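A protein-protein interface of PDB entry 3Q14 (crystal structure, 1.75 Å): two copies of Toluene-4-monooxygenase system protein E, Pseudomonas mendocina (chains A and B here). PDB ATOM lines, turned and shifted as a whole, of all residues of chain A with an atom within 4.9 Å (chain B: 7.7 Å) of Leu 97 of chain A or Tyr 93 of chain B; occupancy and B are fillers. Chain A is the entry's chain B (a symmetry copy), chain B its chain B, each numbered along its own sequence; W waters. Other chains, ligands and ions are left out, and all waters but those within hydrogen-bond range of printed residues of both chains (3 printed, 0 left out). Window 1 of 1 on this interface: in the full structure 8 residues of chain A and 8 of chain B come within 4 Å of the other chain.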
ATOM      1  N   TYR A  93      30.511 -27.670  11.095  1.00  0.00           N
ATOM      2  CA  TYR A  93      30.682 -26.276  10.720  1.00  0.00           C
ATOM      3  C   TYR A  93      32.107 -26.006  10.246  1.00  0.00           C
ATOM      4  O   TYR A  93      32.306 -25.461   9.168  1.00  0.00           O
ATOM      5  CB  TYR A  93      30.311 -25.396  11.918  1.00  0.00           C
ATOM      6  CG  TYR A  93      30.791 -23.977  11.879  1.00  0.00           C
ATOM      7  CD1 TYR A  93      30.251 -23.056  10.977  1.00  0.00           C
ATOM      8  CD2 TYR A  93      31.747 -23.533  12.781  1.00  0.00           C
ATOM      9  CE1 TYR A  93      30.682 -21.744  10.966  1.00  0.00           C
ATOM     10  CE2 TYR A  93      32.179 -22.223  12.782  1.00  0.00           C
ATOM     11  CZ  TYR A  93      31.651 -21.335  11.868  1.00  0.00           C
ATOM     12  OH  TYR A  93      32.092 -20.037  11.877  1.00  0.00           O
ATOM     13  N   VAL A  94      33.097 -26.416  11.033  1.00  0.00           N
ATOM     14  CA  VAL A  94      34.491 -26.231  10.640  1.00  0.00           C
ATOM     15  C   VAL A  94      34.813 -26.961   9.340  1.00  0.00           C
ATOM     16  O   VAL A  94      35.472 -26.420   8.450  1.00  0.00           O
ATOM     17  CB  VAL A  94      35.452 -26.694  11.748  1.00  0.00           C
ATOM     18  CG1 VAL A  94      36.872 -26.832  11.202  1.00  0.00           C
ATOM     19  CG2 VAL A  94      35.409 -25.707  12.921  1.00  0.00           C
ATOM     20  N   GLN A  95      34.357 -28.198   9.225  1.00  0.00           N
ATOM     21  CA  GLN A  95      34.624 -28.963   8.008  1.00  0.00           C
ATOM     22  C   GLN A  95      33.982 -28.295   6.780  1.00  0.00           C
ATOM     23  O   GLN A  95      34.555 -28.290   5.687  1.00  0.00           O
ATOM     24  CB  GLN A  95      34.203 -30.427   8.177  1.00  0.00           C
ATOM     25  CG  GLN A  95      34.926 -31.161   9.349  1.00  0.00           C
ATOM     26  CD  GLN A  95      36.419 -31.417   9.101  1.00  0.00           C
ATOM     27  OE1 GLN A  95      36.793 -32.011   8.089  1.00  0.00           O
ATOM     28  NE2 GLN A  95      37.269 -30.982  10.037  1.00  0.00           N
ATOM     29  N   SER A  96      32.807 -27.694   6.971  1.00  0.00           N
ATOM     30  CA  SER A  96      32.151 -26.915   5.918  1.00  0.00           C
ATOM     31  C   SER A  96      32.925 -25.655   5.548  1.00  0.00           C
ATOM     32  O   SER A  96      32.997 -25.283   4.369  1.00  0.00           O
ATOM     33  CB  SER A  96      30.718 -26.542   6.331  1.00  0.00           C
ATOM     34  OG  SER A  96      29.885 -27.687   6.272  1.00  0.00           O
ATOM     35  N   LEU A  97      33.486 -24.985   6.555  1.00  0.00           N
ATOM     36  CA  LEU A  97      34.369 -23.854   6.297  1.00  0.00           C
ATOM     37  C   LEU A  97      35.576 -24.297   5.468  1.00  0.00           C
ATOM     38  O   LEU A  97      35.937 -23.635   4.496  1.00  0.00           O
ATOM     39  CB  LEU A  97      34.864 -23.232   7.603  1.00  0.00           C
ATOM     40  CG  LEU A  97      33.854 -22.410   8.400  1.00  0.00           C
ATOM     41  CD1 LEU A  97      34.478 -22.020   9.742  1.00  0.00           C
ATOM     42  CD2 LEU A  97      33.421 -21.175   7.610  1.00  0.00           C
ATOM     43  N   PHE A  98      36.213 -25.393   5.875  1.00  0.00           N
ATOM     44  CA  PHE A  98      37.387 -25.897   5.150  1.00  0.00           C
ATOM     45  C   PHE A  98      37.027 -26.135   3.687  1.00  0.00           C
ATOM     46  O   PHE A  98      37.760 -25.735   2.777  1.00  0.00           O
ATOM     47  CB  PHE A  98      37.899 -27.210   5.743  1.00  0.00           C
ATOM     48  CG  PHE A  98      38.633 -27.054   7.051  1.00  0.00           C
ATOM     49  CD1 PHE A  98      39.010 -28.169   7.775  1.00  0.00           C
ATOM     50  CD2 PHE A  98      38.920 -25.797   7.565  1.00  0.00           C
ATOM     51  CE1 PHE A  98      39.694 -28.042   8.983  1.00  0.00           C
ATOM     52  CE2 PHE A  98      39.586 -25.663   8.775  1.00  0.00           C
ATOM     53  CZ  PHE A  98      39.981 -26.787   9.478  1.00  0.00           C
ATOM     54  N   ASP A  99      35.896 -26.801   3.472  1.00  0.00           N
ATOM     55  CA  ASP A  99      35.447 -27.148   2.123  1.00  0.00           C
ATOM     56  C   ASP A  99      35.218 -25.889   1.292  1.00  0.00           C
ATOM     57  O   ASP A  99      35.707 -25.785   0.173  1.00  0.00           O
ATOM     58  CB  ASP A  99      34.178 -27.996   2.202  1.00  0.00           C
ATOM     59  CG  ASP A  99      33.740 -28.526   0.855  1.00  0.00           C
ATOM     60  OD1 ASP A  99      34.591 -28.650  -0.046  1.00  0.00           O
ATOM     61  OD2 ASP A  99      32.539 -28.833   0.705  1.00  0.00           O
ATOM     62  N   GLN A 100      34.487 -24.927   1.851  1.00  0.00           N
ATOM     63  CA  GLN A 100      34.110 -23.722   1.119  1.00  0.00           C
ATOM     64  C   GLN A 100      35.312 -22.824   0.839  1.00  0.00           C
ATOM     65  O   GLN A 100      35.437 -22.269  -0.251  1.00  0.00           O
ATOM     66  CB  GLN A 100      33.033 -22.942   1.883  1.00  0.00           C
ATOM     67  CG  GLN A 100      32.483 -21.748   1.115  1.00  0.00           C
ATOM     68  CD  GLN A 100      32.059 -22.117  -0.296  1.00  0.00           C
ATOM     69  OE1 GLN A 100      31.396 -23.135  -0.517  1.00  0.00           O
ATOM     70  NE2 GLN A 100      32.459 -21.302  -1.265  1.00  0.00           N
ATOM     71  N   PHE A 101      36.193 -22.670   1.821  1.00  0.00           N
ATOM     72  CA  PHE A 101      37.349 -21.806   1.620  1.00  0.00           C
ATOM     73  C   PHE A 101      38.326 -22.402   0.621  1.00  0.00           C
ATOM     74  O   PHE A 101      38.955 -21.685  -0.157  1.00  0.00           O
ATOM     75  CB  PHE A 101      38.017 -21.470   2.948  1.00  0.00           C
ATOM     76  CG  PHE A 101      37.313 -20.376   3.695  1.00  0.00           C
ATOM     77  CD1 PHE A 101      37.915 -19.137   3.867  1.00  0.00           C
ATOM     78  CD2 PHE A 101      36.022 -20.565   4.178  1.00  0.00           C
ATOM     79  CE1 PHE A 101      37.258 -18.115   4.541  1.00  0.00           C
ATOM     80  CE2 PHE A 101      35.356 -19.541   4.853  1.00  0.00           C
ATOM     81  CZ  PHE A 101      35.978 -18.318   5.030  1.00  0.00           C
ATOM     82  N   ASN A 102      38.434 -23.723   0.631  1.00  0.00           N
ATOM     83  CA  ASN A 102      39.225 -24.418  -0.376  1.00  0.00           C
ATOM     84  C   ASN A 102      38.636 -24.225  -1.786  1.00  0.00           C
ATOM     85  O   ASN A 102      39.373 -23.972  -2.746  1.00  0.00           O
ATOM     86  CB  ASN A 102      39.341 -25.903  -0.024  1.00  0.00           C
ATOM     87  CG  ASN A 102      39.981 -26.711  -1.129  1.00  0.00           C
ATOM     88  OD1 ASN A 102      41.200 -26.914  -1.144  1.00  0.00           O
ATOM     89  ND2 ASN A 102      39.168 -27.165  -2.071  1.00  0.00           N
ATOM     90  N   LEU A 246      40.186 -17.484   7.031  1.00  0.00           N
ATOM     91  CA  LEU A 246      39.811 -18.793   7.564  1.00  0.00           C
ATOM     92  C   LEU A 246      40.310 -18.991   8.992  1.00  0.00           C
ATOM     93  O   LEU A 246      39.552 -19.422   9.871  1.00  0.00           O
ATOM     94  CB  LEU A 246      40.342 -19.917   6.666  1.00  0.00           C
ATOM     95  CG  LEU A 246      40.103 -21.365   7.092  1.00  0.00           C
ATOM     96  CD1 LEU A 246      38.617 -21.645   7.355  1.00  0.00           C
ATOM     97  CD2 LEU A 246      40.641 -22.305   6.000  1.00  0.00           C
ATOM     98  N   LEU A 249      38.172 -17.697  11.937  1.00  0.00           N
ATOM     99  CA  LEU A 249      36.938 -18.448  12.148  1.00  0.00           C
ATOM    100  C   LEU A 249      37.255 -19.785  12.800  1.00  0.00           C
ATOM    101  O   LEU A 249      36.532 -20.257  13.679  1.00  0.00           O
ATOM    102  CB  LEU A 249      36.212 -18.674  10.819  1.00  0.00           C
ATOM    103  CG  LEU A 249      35.618 -17.405  10.210  1.00  0.00           C
ATOM    104  CD1 LEU A 249      35.202 -17.639   8.761  1.00  0.00           C
ATOM    105  CD2 LEU A 249      34.434 -16.901  11.047  1.00  0.00           C
ATOM    106  N   GLN B  87      20.612 -31.134   4.167  1.00  0.00           N
ATOM    107  CA  GLN B  87      20.226 -29.767   4.479  1.00  0.00           C
ATOM    108  C   GLN B  87      20.373 -29.435   5.950  1.00  0.00           C
ATOM    109  O   GLN B  87      20.594 -28.287   6.302  1.00  0.00           O
ATOM    110  CB  GLN B  87      18.809 -29.464   3.978  1.00  0.00           C
ATOM    111  CG  GLN B  87      18.710 -29.510   2.449  1.00  0.00           C
ATOM    112  CD  GLN B  87      19.679 -28.562   1.746  1.00  0.00           C
ATOM    113  OE1 GLN B  87      20.878 -28.827   1.664  1.00  0.00           O
ATOM    114  NE2 GLN B  87      19.154 -27.456   1.226  1.00  0.00           N
ATOM    115  N   ASP B  88      20.261 -30.428   6.823  1.00  0.00           N
ATOM    116  CA  ASP B  88      20.522 -30.127   8.223  1.00  0.00           C
ATOM    117  C   ASP B  88      22.002 -29.756   8.352  1.00  0.00           C
ATOM    118  O   ASP B  88      22.376 -28.884   9.147  1.00  0.00           O
ATOM    119  CB  ASP B  88      20.175 -31.302   9.117  1.00  0.00           C
ATOM    120  CG  ASP B  88      20.279 -30.954  10.592  1.00  0.00           C
ATOM    121  OD1 ASP B  88      19.924 -29.811  10.986  1.00  0.00           O
ATOM    122  OD2 ASP B  88      20.728 -31.832  11.351  1.00  0.00           O
ATOM    123  N   GLY B  89      22.835 -30.402   7.546  1.00  0.00           N
ATOM    124  CA  GLY B  89      24.248 -30.070   7.478  1.00  0.00           C
ATOM    125  C   GLY B  89      24.478 -28.645   7.007  1.00  0.00           C
ATOM    126  O   GLY B  89      25.140 -27.857   7.683  1.00  0.00           O
ATOM    127  N   GLN B  90      23.916 -28.304   5.849  1.00  0.00           N
ATOM    128  CA  GLN B  90      24.095 -26.968   5.284  1.00  0.00           C
ATOM    129  C   GLN B  90      23.444 -25.916   6.162  1.00  0.00           C
ATOM    130  O   GLN B  90      23.971 -24.817   6.335  1.00  0.00           O
ATOM    131  CB  GLN B  90      23.527 -26.880   3.860  1.00  0.00           C
ATOM    132  CG  GLN B  90      24.452 -27.402   2.792  1.00  0.00           C
ATOM    133  CD  GLN B  90      25.763 -26.652   2.773  1.00  0.00           C
ATOM    134  OE1 GLN B  90      25.804 -25.440   2.534  1.00  0.00           O
ATOM    135  NE2 GLN B  90      26.839 -27.359   3.066  1.00  0.00           N
ATOM    136  N   GLU B  91      22.283 -26.235   6.716  1.00  0.00           N
ATOM    137  CA  GLU B  91      21.555 -25.239   7.486  1.00  0.00           C
ATOM    138  C   GLU B  91      22.190 -25.042   8.859  1.00  0.00           C
ATOM    139  O   GLU B  91      22.236 -23.924   9.360  1.00  0.00           O
ATOM    140  CB  GLU B  91      20.061 -25.581   7.551  1.00  0.00           C
ATOM    141  CG  GLU B  91      19.151 -24.436   7.962  1.00  0.00           C
ATOM    142  CD  GLU B  91      19.230 -23.185   7.077  1.00  0.00           C
ATOM    143  OE1 GLU B  91      19.819 -23.214   5.977  1.00  0.00           O
ATOM    144  OE2 GLU B  91      18.687 -22.142   7.499  1.00  0.00           O
ATOM    145  N   SER B  92      22.734 -26.107   9.453  1.00  0.00           N
ATOM    146  CA  SER B  92      23.483 -25.949  10.696  1.00  0.00           C
ATOM    147  C   SER B  92      24.700 -25.041  10.475  1.00  0.00           C
ATOM    148  O   SER B  92      25.023 -24.193  11.319  1.00  0.00           O
ATOM    149  CB  SER B  92      23.928 -27.310  11.243  1.00  0.00           C
ATOM    150  OG  SER B  92      24.696 -27.157  12.428  1.00  0.00           O
ATOM    151  N   TYR B  93      25.368 -25.226   9.333  1.00  0.00           N
ATOM    152  CA  TYR B  93      26.506 -24.406   8.955  1.00  0.00           C
ATOM    153  C   TYR B  93      26.111 -22.937   8.837  1.00  0.00           C
ATOM    154  O   TYR B  93      26.743 -22.077   9.436  1.00  0.00           O
ATOM    155  CB  TYR B  93      27.082 -24.942   7.639  1.00  0.00           C
ATOM    156  CG  TYR B  93      27.987 -24.020   6.881  1.00  0.00           C
ATOM    157  CD1 TYR B  93      29.260 -23.702   7.361  1.00  0.00           C
ATOM    158  CD2 TYR B  93      27.598 -23.505   5.653  1.00  0.00           C
ATOM    159  CE1 TYR B  93      30.098 -22.870   6.643  1.00  0.00           C
ATOM    160  CE2 TYR B  93      28.430 -22.680   4.924  1.00  0.00           C
ATOM    161  CZ  TYR B  93      29.674 -22.359   5.427  1.00  0.00           C
ATOM    162  OH  TYR B  93      30.489 -21.535   4.695  1.00  0.00           O
ATOM    163  N   VAL B  94      25.046 -22.653   8.092  1.00  0.00           N
ATOM    164  CA  VAL B  94      24.576 -21.277   7.954  1.00  0.00           C
ATOM    165  C   VAL B  94      24.176 -20.679   9.299  1.00  0.00           C
ATOM    166  O   VAL B  94      24.513 -19.537   9.616  1.00  0.00           O
ATOM    167  CB  VAL B  94      23.395 -21.185   6.972  1.00  0.00           C
ATOM    168  CG1 VAL B  94      22.693 -19.835   7.106  1.00  0.00           C
ATOM    169  CG2 VAL B  94      23.893 -21.405   5.538  1.00  0.00           C
ATOM    170  N   GLN B  95      23.447 -21.444  10.096  1.00  0.00           N
ATOM    171  CA  GLN B  95      23.024 -20.942  11.401  1.00  0.00           C
ATOM    172  C   GLN B  95      24.237 -20.647  12.302  1.00  0.00           C
ATOM    173  O   GLN B  95      24.242 -19.674  13.062  1.00  0.00           O
ATOM    174  CB  GLN B  95      22.016 -21.893  12.056  1.00  0.00           C
ATOM    175  CG  GLN B  95      20.724 -22.121  11.211  1.00  0.00           C
ATOM    176  CD  GLN B  95      19.806 -20.894  11.129  1.00  0.00           C
ATOM    177  OE1 GLN B  95      19.409 -20.338  12.153  1.00  0.00           O
ATOM    178  NE2 GLN B  95      19.456 -20.484   9.904  1.00  0.00           N
ATOM    179  N   SER B  96      25.283 -21.465  12.185  1.00  0.00           N
ATOM    180  CA  SER B  96      26.544 -21.222  12.890  1.00  0.00           C
ATOM    181  C   SER B  96      27.258 -19.966  12.403  1.00  0.00           C
ATOM    182  O   SER B  96      27.845 -19.226  13.203  1.00  0.00           O
ATOM    183  CB  SER B  96      27.480 -22.435  12.763  1.00  0.00           C
ATOM    184  OG  SER B  96      27.006 -23.497  13.573  1.00  0.00           O
ATOM    185  N   LEU B  97      27.229 -19.738  11.090  1.00  0.00           N
ATOM    186  CA  LEU B  97      27.752 -18.494  10.539  1.00  0.00           C
ATOM    187  C   LEU B  97      26.993 -17.295  11.111  1.00  0.00           C
ATOM    188  O   LEU B  97      27.606 -16.311  11.523  1.00  0.00           O
ATOM    189  CB  LEU B  97      27.637 -18.473   9.015  1.00  0.00           C
ATOM    190  CG  LEU B  97      28.610 -19.360   8.240  1.00  0.00           C
ATOM    191  CD1 LEU B  97      28.229 -19.338   6.757  1.00  0.00           C
ATOM    192  CD2 LEU B  97      30.049 -18.894   8.450  1.00  0.00           C
ATOM    193  N   PHE B  98      25.663 -17.368  11.102  1.00  0.00           N
ATOM    194  CA  PHE B  98      24.842 -16.267  11.624  1.00  0.00           C
ATOM    195  C   PHE B  98      25.241 -15.965  13.066  1.00  0.00           C
ATOM    196  O   PHE B  98      25.431 -14.806  13.444  1.00  0.00           O
ATOM    197  CB  PHE B  98      23.352 -16.608  11.594  1.00  0.00           C
ATOM    198  CG  PHE B  98      22.736 -16.566  10.218  1.00  0.00           C
ATOM    199  CD1 PHE B  98      21.440 -17.004  10.023  1.00  0.00           C
ATOM    200  CD2 PHE B  98      23.459 -16.115   9.123  1.00  0.00           C
ATOM    201  CE1 PHE B  98      20.852 -16.966   8.759  1.00  0.00           C
ATOM    202  CE2 PHE B  98      22.886 -16.092   7.859  1.00  0.00           C
ATOM    203  CZ  PHE B  98      21.580 -16.508   7.681  1.00  0.00           C
ATOM    204  N   ASP B  99      25.353 -17.021  13.866  1.00  0.00           N
ATOM    205  CA  ASP B  99      25.678 -16.883  15.286  1.00  0.00           C
ATOM    206  C   ASP B  99      27.042 -16.224  15.465  1.00  0.00           C
ATOM    207  O   ASP B  99      27.178 -15.271  16.224  1.00  0.00           O
ATOM    208  CB  ASP B  99      25.634 -18.253  15.963  1.00  0.00           C
ATOM    209  CG  ASP B  99      25.805 -18.174  17.463  1.00  0.00           C
ATOM    210  OD1 ASP B  99      25.508 -17.113  18.045  1.00  0.00           O
ATOM    211  OD2 ASP B  99      26.226 -19.186  18.062  1.00  0.00           O
ATOM    212  N   GLN B 100      28.047 -16.724  14.748  1.00  0.00           N
ATOM    213  CA  GLN B 100      29.418 -16.249  14.908  1.00  0.00           C
ATOM    214  C   GLN B 100      29.592 -14.822  14.397  1.00  0.00           C
ATOM    215  O   GLN B 100      30.275 -14.013  15.021  1.00  0.00           O
ATOM    216  CB  GLN B 100      30.400 -17.190  14.199  1.00  0.00           C
ATOM    217  CG  GLN B 100      31.862 -16.842  14.441  1.00  0.00           C
ATOM    218  CD  GLN B 100      32.174 -16.663  15.918  1.00  0.00           C
ATOM    219  OE1 GLN B 100      31.759 -17.467  16.759  1.00  0.00           O
ATOM    220  NE2 GLN B 100      32.889 -15.594  16.245  1.00  0.00           N
ATOM    221  N   PHE B 101      28.987 -14.510  13.256  1.00  0.00           N
ATOM    222  CA  PHE B 101      29.136 -13.169  12.706  1.00  0.00           C
ATOM    223  C   PHE B 101      28.419 -12.134  13.555  1.00  0.00           C
ATOM    224  O   PHE B 101      28.883 -11.004  13.704  1.00  0.00           O
ATOM    225  CB  PHE B 101      28.693 -13.125  11.248  1.00  0.00           C
ATOM    226  CG  PHE B 101      29.738 -13.642  10.305  1.00  0.00           C
ATOM    227  CD1 PHE B 101      30.377 -12.785   9.419  1.00  0.00           C
ATOM    228  CD2 PHE B 101      30.127 -14.977  10.341  1.00  0.00           C
ATOM    229  CE1 PHE B 101      31.360 -13.256   8.558  1.00  0.00           C
ATOM    230  CE2 PHE B 101      31.116 -15.455   9.480  1.00  0.00           C
ATOM    231  CZ  PHE B 101      31.730 -14.591   8.592  1.00  0.00           C
ATOM    232  N   ARG B 161      13.658 -22.157   2.161  1.00  0.00           N
ATOM    233  CA  ARG B 161      14.908 -22.003   2.902  1.00  0.00           C
ATOM    234  C   ARG B 161      15.504 -20.620   2.603  1.00  0.00           C
ATOM    235  O   ARG B 161      15.864 -19.881   3.515  1.00  0.00           O
ATOM    236  CB  ARG B 161      15.890 -23.123   2.539  1.00  0.00           C
ATOM    237  CG  ARG B 161      17.270 -22.933   3.151  1.00  0.00           C
ATOM    238  CD  ARG B 161      18.290 -23.976   2.633  1.00  0.00           C
ATOM    239  NE  ARG B 161      19.505 -23.870   3.436  1.00  0.00           N
ATOM    240  CZ  ARG B 161      20.735 -23.690   2.961  1.00  0.00           C
ATOM    241  NH1 ARG B 161      21.755 -23.586   3.809  1.00  0.00           N
ATOM    242  NH2 ARG B 161      20.959 -23.631   1.651  1.00  0.00           N
ATOM    243  N   LEU B 246      29.656 -11.819   5.363  1.00  0.00           N
ATOM    244  CA  LEU B 246      28.648 -12.846   5.626  1.00  0.00           C
ATOM    245  C   LEU B 246      27.835 -13.179   4.379  1.00  0.00           C
ATOM    246  O   LEU B 246      27.641 -14.356   4.047  1.00  0.00           O
ATOM    247  CB  LEU B 246      27.711 -12.409   6.758  1.00  0.00           C
ATOM    248  CG  LEU B 246      26.549 -13.328   7.138  1.00  0.00           C
ATOM    249  CD1 LEU B 246      27.027 -14.751   7.454  1.00  0.00           C
ATOM    250  CD2 LEU B 246      25.810 -12.728   8.346  1.00  0.00           C
ATOM    251  N   PRO B 248      28.408 -13.152   1.169  1.00  0.00           N
ATOM    252  CA  PRO B 248      28.972 -14.063   0.159  1.00  0.00           C
ATOM    253  C   PRO B 248      28.959 -15.539   0.600  1.00  0.00           C
ATOM    254  O   PRO B 248      28.741 -16.419  -0.230  1.00  0.00           O
ATOM    255  CB  PRO B 248      30.406 -13.555  -0.016  1.00  0.00           C
ATOM    256  CG  PRO B 248      30.357 -12.118   0.394  1.00  0.00           C
ATOM    257  CD  PRO B 248      29.336 -12.057   1.507  1.00  0.00           C
ATOM    258  N   LEU B 249      29.187 -15.802   1.886  1.00  0.00           N
ATOM    259  CA  LEU B 249      29.167 -17.169   2.397  1.00  0.00           C
ATOM    260  C   LEU B 249      27.743 -17.703   2.382  1.00  0.00           C
ATOM    261  O   LEU B 249      27.498 -18.867   2.060  1.00  0.00           O
ATOM    262  CB  LEU B 249      29.729 -17.221   3.820  1.00  0.00           C
ATOM    263  CG  LEU B 249      31.231 -16.955   3.906  1.00  0.00           C
ATOM    264  CD1 LEU B 249      31.658 -16.703   5.350  1.00  0.00           C
ATOM    265  CD2 LEU B 249      32.026 -18.117   3.293  1.00  0.00           C
ATOM    266  N   LEU B 250      26.793 -16.841   2.730  1.00  0.00           N
ATOM    267  CA  LEU B 250      25.394 -17.248   2.716  1.00  0.00           C
ATOM    268  C   LEU B 250      24.984 -17.588   1.293  1.00  0.00           C
ATOM    269  O   LEU B 250      24.398 -18.640   1.044  1.00  0.00           O
ATOM    270  CB  LEU B 250      24.494 -16.131   3.259  1.00  0.00           C
ATOM    271  CG  LEU B 250      22.986 -16.372   3.154  1.00  0.00           C
ATOM    272  CD1 LEU B 250      22.583 -17.629   3.917  1.00  0.00           C
ATOM    273  CD2 LEU B 250      22.207 -15.150   3.668  1.00  0.00           C
ATOM    274  N   ASP B 252      26.810 -18.427  -1.150  1.00  0.00           N
ATOM    275  CA  ASP B 252      27.479 -19.641  -1.612  1.00  0.00           C
ATOM    276  C   ASP B 252      26.677 -20.885  -1.204  1.00  0.00           C
ATOM    277  O   ASP B 252      26.590 -21.844  -1.964  1.00  0.00           O
ATOM    278  CB  ASP B 252      28.925 -19.721  -1.115  1.00  0.00           C
ATOM    279  CG  ASP B 252      29.915 -19.041  -2.054  1.00  0.00           C
ATOM    280  OD1 ASP B 252      29.563 -18.759  -3.219  1.00  0.00           O
ATOM    281  OD2 ASP B 252      31.066 -18.802  -1.626  1.00  0.00           O
ATOM    282  N   SER B 253      26.080 -20.871  -0.015  1.00  0.00           N
ATOM    283  CA  SER B 253      25.249 -21.997   0.404  1.00  0.00           C
ATOM    284  C   SER B 253      23.957 -22.092  -0.417  1.00  0.00           C
ATOM    285  O   SER B 253      23.514 -23.177  -0.801  1.00  0.00           O
ATOM    286  CB  SER B 253      24.932 -21.917   1.904  1.00  0.00           C
ATOM    287  OG  SER B 253      24.177 -23.050   2.311  1.00  0.00           O
ATOM    288  N   LYS B 256      24.573 -23.649  -3.795  1.00  0.00           N
ATOM    289  CA  LYS B 256      24.633 -25.109  -3.826  1.00  0.00           C
ATOM    290  C   LYS B 256      23.248 -25.674  -4.132  1.00  0.00           C
ATOM    291  O   LYS B 256      23.108 -26.611  -4.927  1.00  0.00           O
ATOM    292  CB  LYS B 256      25.171 -25.691  -2.508  1.00  0.00           C
ATOM    293  CG  LYS B 256      26.648 -25.467  -2.289  1.00  0.00           C
ATOM    294  CD  LYS B 256      27.029 -25.833  -0.855  1.00  0.00           C
ATOM    295  CE  LYS B 256      28.537 -25.935  -0.675  1.00  0.00           C
ATOM    296  NZ  LYS B 256      29.022 -27.332  -0.869  1.00  0.00           N
HETATM  297  O   HOH W   1      27.238 -27.021  11.994  1.00  0.00           O
HETATM  298  O   HOH W   2      31.579 -26.142  -0.159  1.00  0.00           O
HETATM  299  O   HOH W   3      27.503 -29.568   4.749  1.00  0.00           O
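The backbone carbonyl oxygen of Ser 92 of chain B is in hydrogen-bond range of the side-chain hydroxyl of Ser 96 of chain B (3.1 Å).
Of the 23 printed residues of chain B, 6 touch a printed residue of chain A. Printed residues of chain B that touch a printed residue of chain A: Tyr 93, Ser 96, Leu 97, Phe 101, Leu 249 and Asp 252.
Tyr 93 of chain B touches its own counterpart, Tyr 93 of chain A. Tyr 93 of chain A touches Ser 96 of chain B, and with the chains exchanged Ser 96 of chain A touches Tyr 93 of chain B. Tyr 93 of chain A touches Leu 97 of chain B, and with the chains exchanged Leu 97 of chain A touches Tyr 93 of chain B. Phe 101 of chain A touches Leu 249 of chain B, and with the chains exchanged Leu 249 of chain A touches Phe 101 of chain B. Positions printed for both chains: 93, 94, 95, 96, 97, 98, 99, 100, 101, 246 and 249. Of the 8 pairs that touch across the chains among the printed residues, 7 have their exchanged pair printed and touching as well.
The side-chain amide nitrogen (NE2) of Gln 100 of chain A sits at hydrogen-bond distance from the side-chain carboxylate (OD2) of Asp 252 of chain B.
Among the printed residues, pairs that only touch across the chains: Ser 96 of chain A with Tyr 93 of chain B (3.4 Å), Tyr 93 of chain A with Ser 96 of chain B (3.4 Å), Tyr 93 of chain A with Tyr 93 of chain B (3.8 Å), Leu 97 of chain A with Tyr 93 of chain B (3.9 Å), Tyr 93 of chain A with Leu 97 of chain B (3.9 Å), Phe 101 of chain A with Leu 249 of chain B (3.9 Å) and Leu 249 of chain A with Phe 101 of chain B (3.9 Å).
Of the printed residues of chain B, Leu 97 of chain A touches Tyr 93 (3.9 Å). Of chain A, only Tyr 93, Ser 96 and Leu 97 come within 4 Å of Tyr 93 of chain B. Printed residues of chain B within 4 Å of Gln 100 of chain A: Asp 252. Of the printed residues of chain B, Phe 101 of chain A touches Leu 249 (3.9 Å). Of the printed residues of chain A, Asp 252 of chain B touches Gln 100 (2.9 Å). Of the printed residues of chain B, Ser 96 of chain A touches Tyr 93. The nearest residue of chain B that does not touch Leu 97 of chain A is Leu 97 of chain B (4.2 Å). The nearest residue of chain A that does not touch Tyr 93 of chain B is Gln 100 of chain A (4.04 Å). The nearest printed residue of chain B that does not touch Ser 96 of chain A is Gln 90 of chain B (4.4 Å).
Water W1 lies within hydrogen-bond range of OG of Ser 92 of chain B (2.6 Å) and N of Tyr 93 of chain A (3.5 Å). Water W3 bridges NE2 of Gln 90 of chain B and OG of Ser 96 of chain A. Water W2 lies within hydrogen-bond range of NZ of Lys 256 of chain B, OD2 of Asp 99 of chain A and OE1 of Gln 100 of chain A.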
